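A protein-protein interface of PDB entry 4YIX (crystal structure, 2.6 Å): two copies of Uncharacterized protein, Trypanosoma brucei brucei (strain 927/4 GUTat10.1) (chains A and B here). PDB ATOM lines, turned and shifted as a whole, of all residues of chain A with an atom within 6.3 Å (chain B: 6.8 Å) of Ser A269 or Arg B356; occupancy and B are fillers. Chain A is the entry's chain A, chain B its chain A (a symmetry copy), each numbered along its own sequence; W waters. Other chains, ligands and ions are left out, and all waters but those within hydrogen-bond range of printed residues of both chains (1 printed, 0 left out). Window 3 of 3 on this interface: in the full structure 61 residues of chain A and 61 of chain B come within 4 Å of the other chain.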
ATOM      1  N   ARG A 264      11.487  20.277  -4.008  1.00  0.00           N
ATOM      2  CA  ARG A 264      12.601  19.948  -4.877  1.00  0.00           C
ATOM      3  C   ARG A 264      12.074  19.654  -6.280  1.00  0.00           C
ATOM      4  O   ARG A 264      10.865  19.523  -6.491  1.00  0.00           O
ATOM      5  CB  ARG A 264      13.388  18.759  -4.324  1.00  0.00           C
ATOM      6  CG  ARG A 264      13.903  18.947  -2.904  1.00  0.00           C
ATOM      7  CD  ARG A 264      14.937  20.068  -2.798  1.00  0.00           C
ATOM      8  NE  ARG A 264      14.316  21.377  -2.608  1.00  0.00           N
ATOM      9  CZ  ARG A 264      14.967  22.538  -2.634  1.00  0.00           C
ATOM     10  NH1 ARG A 264      16.277  22.581  -2.849  1.00  0.00           N
ATOM     11  NH2 ARG A 264      14.297  23.664  -2.448  1.00  0.00           N
ATOM     12  N   ASP A 265      12.989  19.552  -7.235  1.00  0.00           N
ATOM     13  CA  ASP A 265      12.620  19.512  -8.636  1.00  0.00           C
ATOM     14  C   ASP A 265      12.181  18.130  -9.099  1.00  0.00           C
ATOM     15  O   ASP A 265      11.517  18.000 -10.117  1.00  0.00           O
ATOM     16  CB  ASP A 265      13.792  19.986  -9.488  1.00  0.00           C
ATOM     17  CG  ASP A 265      13.380  20.333 -10.897  1.00  0.00           C
ATOM     18  OD1 ASP A 265      12.250  20.838 -11.082  1.00  0.00           O
ATOM     19  OD2 ASP A 265      14.187  20.100 -11.820  1.00  0.00           O
ATOM     20  N   ALA A 266      12.569  17.099  -8.359  1.00  0.00           N
ATOM     21  CA  ALA A 266      12.214  15.730  -8.697  1.00  0.00           C
ATOM     22  C   ALA A 266      12.399  14.845  -7.479  1.00  0.00           C
ATOM     23  O   ALA A 266      12.956  15.273  -6.480  1.00  0.00           O
ATOM     24  CB  ALA A 266      13.058  15.225  -9.851  1.00  0.00           C
ATOM     25  N   GLY A 267      11.951  13.601  -7.567  1.00  0.00           N
ATOM     26  CA  GLY A 267      12.082  12.685  -6.450  1.00  0.00           C
ATOM     27  C   GLY A 267      13.516  12.360  -6.092  1.00  0.00           C
ATOM     28  O   GLY A 267      13.828  12.064  -4.947  1.00  0.00           O
ATOM     29  N   ASN A 268      14.391  12.406  -7.086  1.00  0.00           N
ATOM     30  CA  ASN A 268      15.793  12.109  -6.870  1.00  0.00           C
ATOM     31  C   ASN A 268      16.670  13.319  -7.133  1.00  0.00           C
ATOM     32  O   ASN A 268      17.820  13.191  -7.536  1.00  0.00           O
ATOM     33  CB  ASN A 268      16.224  10.953  -7.748  1.00  0.00           C
ATOM     34  CG  ASN A 268      16.053  11.248  -9.223  1.00  0.00           C
ATOM     35  OD1 ASN A 268      15.433  12.238  -9.608  1.00  0.00           O
ATOM     36  ND2 ASN A 268      16.591  10.372 -10.061  1.00  0.00           N
ATOM     37  N   SER A 269      16.124  14.503  -6.901  1.00  0.00           N
ATOM     38  CA  SER A 269      16.902  15.721  -7.042  1.00  0.00           C
ATOM     39  C   SER A 269      16.924  16.480  -5.718  1.00  0.00           C
ATOM     40  O   SER A 269      16.040  16.307  -4.877  1.00  0.00           O
ATOM     41  CB  SER A 269      16.331  16.591  -8.158  1.00  0.00           C
ATOM     42  OG  SER A 269      17.076  17.786  -8.309  1.00  0.00           O
ATOM     43  N   ASP A 270      17.948  17.301  -5.521  1.00  0.00           N
ATOM     44  CA  ASP A 270      17.991  18.174  -4.359  1.00  0.00           C
ATOM     45  C   ASP A 270      17.997  19.626  -4.809  1.00  0.00           C
ATOM     46  O   ASP A 270      18.268  20.526  -4.026  1.00  0.00           O
ATOM     47  CB  ASP A 270      19.215  17.881  -3.491  1.00  0.00           C
ATOM     48  CG  ASP A 270      19.093  18.463  -2.092  1.00  0.00           C
ATOM     49  OD1 ASP A 270      17.978  18.460  -1.530  1.00  0.00           O
ATOM     50  OD2 ASP A 270      20.113  18.927  -1.549  1.00  0.00           O
ATOM     51  N   LYS A 271      17.705  19.850  -6.083  1.00  0.00           N
ATOM     52  CA  LYS A 271      17.589  21.211  -6.580  1.00  0.00           C
ATOM     53  C   LYS A 271      16.148  21.697  -6.435  1.00  0.00           C
ATOM     54  O   LYS A 271      15.216  20.898  -6.455  1.00  0.00           O
ATOM     55  CB  LYS A 271      18.051  21.290  -8.031  1.00  0.00           C
ATOM     56  CG  LYS A 271      19.503  20.904  -8.224  1.00  0.00           C
ATOM     57  CD  LYS A 271      20.052  21.555  -9.466  1.00  0.00           C
ATOM     58  CE  LYS A 271      21.508  21.213  -9.682  1.00  0.00           C
ATOM     59  NZ  LYS A 271      21.668  19.801 -10.132  1.00  0.00           N
ATOM     60  N   PRO A 272      15.962  23.012  -6.274  1.00  0.00           N
ATOM     61  CA  PRO A 272      14.625  23.604  -6.110  1.00  0.00           C
ATOM     62  C   PRO A 272      13.698  23.348  -7.302  1.00  0.00           C
ATOM     63  O   PRO A 272      14.160  23.170  -8.423  1.00  0.00           O
ATOM     64  CB  PRO A 272      14.925  25.098  -5.970  1.00  0.00           C
ATOM     65  CG  PRO A 272      16.235  25.283  -6.639  1.00  0.00           C
ATOM     66  CD  PRO A 272      17.012  24.040  -6.365  1.00  0.00           C
ATOM     67  N   ARG A 324      11.260  18.212   5.553  1.00  0.00           N
ATOM     68  CA  ARG A 324      12.550  17.898   4.969  1.00  0.00           C
ATOM     69  C   ARG A 324      13.473  19.112   5.011  1.00  0.00           C
ATOM     70  O   ARG A 324      14.610  19.030   5.476  1.00  0.00           O
ATOM     71  CB  ARG A 324      12.381  17.408   3.539  1.00  0.00           C
ATOM     72  CG  ARG A 324      11.923  15.978   3.422  1.00  0.00           C
ATOM     73  CD  ARG A 324      11.793  15.544   1.960  1.00  0.00           C
ATOM     74  NE  ARG A 324      10.888  14.409   1.883  1.00  0.00           N
ATOM     75  CZ  ARG A 324       9.782  14.362   1.152  1.00  0.00           C
ATOM     76  NH1 ARG A 324       9.443  15.378   0.371  1.00  0.00           N
ATOM     77  NH2 ARG A 324       9.029  13.273   1.183  1.00  0.00           N
ATOM     78  N   GLU B 354       6.074   4.667  -0.320  1.00  0.00           N
ATOM     79  CA  GLU B 354       7.361   4.854  -0.976  1.00  0.00           C
ATOM     80  C   GLU B 354       7.667   6.266  -1.402  1.00  0.00           C
ATOM     81  O   GLU B 354       7.751   6.557  -2.563  1.00  0.00           O
ATOM     82  CB  GLU B 354       7.505   3.909  -2.142  1.00  0.00           C
ATOM     83  CG  GLU B 354       8.878   3.837  -2.732  1.00  0.00           C
ATOM     84  CD  GLU B 354       8.966   2.921  -3.890  1.00  0.00           C
ATOM     85  OE1 GLU B 354       8.172   2.056  -3.994  1.00  0.00           O
ATOM     86  OE2 GLU B 354       9.800   3.105  -4.718  1.00  0.00           O
ATOM     87  N   ASP B 355       7.934   7.131  -0.461  1.00  0.00           N
ATOM     88  CA  ASP B 355       8.031   8.540  -0.699  1.00  0.00           C
ATOM     89  C   ASP B 355       9.037   8.942  -1.716  1.00  0.00           C
ATOM     90  O   ASP B 355      10.115   8.474  -1.732  1.00  0.00           O
ATOM     91  CB  ASP B 355       8.523   9.173   0.565  1.00  0.00           C
ATOM     92  CG  ASP B 355       7.590  10.148   1.145  1.00  0.00           C
ATOM     93  OD1 ASP B 355       7.417  11.232   0.604  1.00  0.00           O
ATOM     94  OD2 ASP B 355       7.097   9.831   2.221  1.00  0.00           O
ATOM     95  N   ARG B 356       8.653   9.873  -2.552  1.00  0.00           N
ATOM     96  CA  ARG B 356       9.536  10.511  -3.470  1.00  0.00           C
ATOM     97  C   ARG B 356       9.763   9.761  -4.736  1.00  0.00           C
ATOM     98  O   ARG B 356      10.486  10.191  -5.524  1.00  0.00           O
ATOM     99  CB  ARG B 356      10.884  10.814  -2.830  1.00  0.00           C
ATOM    100  CG  ARG B 356      10.920  11.708  -1.629  1.00  0.00           C
ATOM    101  CD  ARG B 356      11.117  13.114  -2.034  1.00  0.00           C
ATOM    102  NE  ARG B 356      12.476  13.562  -1.962  1.00  0.00           N
ATOM    103  CZ  ARG B 356      12.930  14.577  -2.641  1.00  0.00           C
ATOM    104  NH1 ARG B 356      12.157  15.228  -3.407  1.00  0.00           N
ATOM    105  NH2 ARG B 356      14.159  14.936  -2.540  1.00  0.00           N
ATOM    106  N   ARG B 357       9.121   8.626  -4.901  1.00  0.00           N
ATOM    107  CA  ARG B 357       9.205   7.814  -6.111  1.00  0.00           C
ATOM    108  C   ARG B 357       8.434   8.483  -7.231  1.00  0.00           C
ATOM    109  O   ARG B 357       7.596   9.328  -6.971  1.00  0.00           O
ATOM    110  CB  ARG B 357       8.667   6.406  -5.871  1.00  0.00           C
ATOM    111  CG  ARG B 357       7.175   6.349  -5.656  1.00  0.00           C
ATOM    112  CD  ARG B 357       6.603   4.997  -6.052  1.00  0.00           C
ATOM    113  NE  ARG B 357       6.554   4.791  -7.497  1.00  0.00           N
ATOM    114  CZ  ARG B 357       5.795   3.877  -8.097  1.00  0.00           C
ATOM    115  NH1 ARG B 357       5.014   3.078  -7.381  1.00  0.00           N
ATOM    116  NH2 ARG B 357       5.803   3.766  -9.417  1.00  0.00           N
ATOM    117  N   SER B 358       8.711   8.110  -8.476  1.00  0.00           N
ATOM    118  CA  SER B 358       7.951   8.654  -9.594  1.00  0.00           C
ATOM    119  C   SER B 358       6.870   7.683 -10.055  1.00  0.00           C
ATOM    120  O   SER B 358       6.982   6.474  -9.871  1.00  0.00           O
ATOM    121  CB  SER B 358       8.866   9.014 -10.767  1.00  0.00           C
ATOM    122  OG  SER B 358       9.397   7.870 -11.407  1.00  0.00           O
ATOM    123  N   ALA B 383       6.832  13.209 -10.479  1.00  0.00           N
ATOM    124  CA  ALA B 383       8.220  12.930 -10.265  1.00  0.00           C
ATOM    125  C   ALA B 383       8.578  12.862  -8.786  1.00  0.00           C
ATOM    126  O   ALA B 383       9.683  12.663  -8.460  1.00  0.00           O
ATOM    127  CB  ALA B 383       9.046  13.982 -10.941  1.00  0.00           C
ATOM    128  N   ASP B 384       7.646  13.109  -7.908  1.00  0.00           N
ATOM    129  CA  ASP B 384       7.910  13.162  -6.493  1.00  0.00           C
ATOM    130  C   ASP B 384       6.699  12.781  -5.697  1.00  0.00           C
ATOM    131  O   ASP B 384       5.956  13.621  -5.286  1.00  0.00           O
ATOM    132  CB  ASP B 384       8.320  14.573  -6.171  1.00  0.00           C
ATOM    133  CG  ASP B 384       9.308  14.676  -5.118  1.00  0.00           C
ATOM    134  OD1 ASP B 384       9.334  13.927  -4.207  1.00  0.00           O
ATOM    135  OD2 ASP B 384      10.054  15.606  -5.182  1.00  0.00           O
ATOM    136  N   ALA B 385       6.495  11.514  -5.500  1.00  0.00           N
ATOM    137  CA  ALA B 385       5.346  11.043  -4.788  1.00  0.00           C
ATOM    138  C   ALA B 385       5.450  11.345  -3.336  1.00  0.00           C
ATOM    139  O   ALA B 385       6.501  11.417  -2.791  1.00  0.00           O
ATOM    140  CB  ALA B 385       5.071   9.578  -5.054  1.00  0.00           C
ATOM    141  N   SER B 386       4.306  11.552  -2.740  1.00  0.00           N
ATOM    142  CA  SER B 386       4.212  11.665  -1.298  1.00  0.00           C
ATOM    143  C   SER B 386       4.008  10.266  -0.723  1.00  0.00           C
ATOM    144  O   SER B 386       3.988   9.288  -1.466  1.00  0.00           O
ATOM    145  CB  SER B 386       3.059  12.593  -0.903  1.00  0.00           C
ATOM    146  OG  SER B 386       1.803  11.962  -1.101  1.00  0.00           O
ATOM    147  N   GLY B 387       3.846  10.165   0.590  1.00  0.00           N
ATOM    148  CA  GLY B 387       3.632   8.873   1.217  1.00  0.00           C
ATOM    149  C   GLY B 387       2.323   8.218   0.804  1.00  0.00           C
ATOM    150  O   GLY B 387       2.288   7.039   0.491  1.00  0.00           O
ATOM    151  N   SER B 390       2.093   7.513  -3.245  1.00  0.00           N
ATOM    152  CA  SER B 390       3.013   6.471  -3.687  1.00  0.00           C
ATOM    153  C   SER B 390       2.487   5.113  -3.283  1.00  0.00           C
ATOM    154  O   SER B 390       2.656   4.133  -4.000  1.00  0.00           O
ATOM    155  CB  SER B 390       4.404   6.665  -3.095  1.00  0.00           C
ATOM    156  OG  SER B 390       4.472   6.111  -1.797  1.00  0.00           O
ATOM    157  N   ARG B 659      12.265   6.636 -14.130  1.00  0.00           N
ATOM    158  CA  ARG B 659      11.846   8.025 -14.018  1.00  0.00           C
ATOM    159  C   ARG B 659      11.580   8.678 -15.365  1.00  0.00           C
ATOM    160  O   ARG B 659      10.917   9.703 -15.434  1.00  0.00           O
ATOM    161  CB  ARG B 659      12.877   8.817 -13.223  1.00  0.00           C
ATOM    162  CG  ARG B 659      12.786   8.523 -11.740  1.00  0.00           C
ATOM    163  CD  ARG B 659      13.729   9.361 -10.909  1.00  0.00           C
ATOM    164  NE  ARG B 659      13.476   9.149  -9.486  1.00  0.00           N
ATOM    165  CZ  ARG B 659      12.524   9.772  -8.800  1.00  0.00           C
ATOM    166  NH1 ARG B 659      11.744  10.658  -9.401  1.00  0.00           N
ATOM    167  NH2 ARG B 659      12.355   9.514  -7.515  1.00  0.00           N
HETATM  168  O   HOH W   1       7.191  13.807  -1.770  1.00  0.00           O
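The backbone carbonyl oxygen (O) of Ser A269 lies within hydrogen-bond range of the guanidinium group (NH2) of Arg B356, at 3.3 Å. N of Gly A267 sits at hydrogen-bond distance from O of Ala B383, 2.6 Å away. The backbone NH (N) of Gly A267 lies close to the guanidinium group (NH1) of Arg B659 (3.5 Å). O of Ala A266 sits close to OD2 of Asp B384 (3.2 Å). The guanidinium group (NH1) of Arg B356 lies within hydrogen-bond range of the backbone carbonyl oxygen (O) of Ala A266 (3.2 Å). ND2 of Asn A268 lies close to NE of Arg B659, 3.4 Å away. The guanidinium group of Arg A324 is in salt-bridge range of the side-chain carboxylate of Asp B355, 2.7 Å away.
NH1 of Arg B356 lies within salt-bridge range of OD2 of Asp B384, at 2.8 Å. The backbone carbonyl oxygen (O) of Asp A270 is in hydrogen-bond range of the guanidinium group (NH1) of Arg A264, 3.1 Å away. NH2 of Arg B659 is in hydrogen-bond range of O of Arg B356, 2.8 Å away. The side-chain hydroxyl (OG) of Ser A269 lies within hydrogen-bond range of the backbone NH (N) of Lys A271 (3.1 Å). The backbone NH (N) of Arg B356 is in hydrogen-bond range of the backbone carbonyl oxygen (O) of Ala B385 (2.7 Å). O of Ala B383 sits at hydrogen-bond distance from NH1 of Arg B659.
Among the printed residues, pairs that only touch across the chains: Arg A264 with Arg B356 (3.9 Å), Ala A266 with Ala B383 (3.6 Å), Gly A267 with Arg B356 (3.1 Å), Gly A267 with Asp B384 (3.6 Å) and Arg A324 with Arg B356 (3.7 Å).
Of chain B, only Arg B356 (3.3 Å) comes within 4 Å of Ser A269. Arg B356 touches just these residues of chain A: Arg A264 (3.9 Å), Ala A266 (3.2 Å), Gly A267 (3.1 Å), Ser A269 (3.3 Å) and Arg A324 (3.7 Å). Printed residues of chain B within 4 Å of Ala A266: Arg B356, Ala B383 and Asp B384. Of the printed residues of chain B, Arg A324 touches Asp B355 and Arg B356. The nearest residue of chain B that does not touch Ser A269 is Asp B384 (6.0 Å). The nearest residue of chain A that does not touch Arg B356 is Asn A268 (4.8 Å). The nearest printed residue of chain B that does not touch Asn A268 is Arg B356 (4.8 Å).
Along chain B the printed residues that touch a printed residue of chain A span positions 355 to 659. Among the printed residues, 12 pairs touch across the chains.
No position is printed for both chains. Of the 12 pairs that touch across the chains among the printed residues, none has its exchanged pair printed and touching as well.
Water W1 lies within hydrogen-bond range of O of Ala B385 (2.7 Å), OD1 of Asp B384 (3.2 Å) and NH1 of Arg A324 (3.5 Å).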
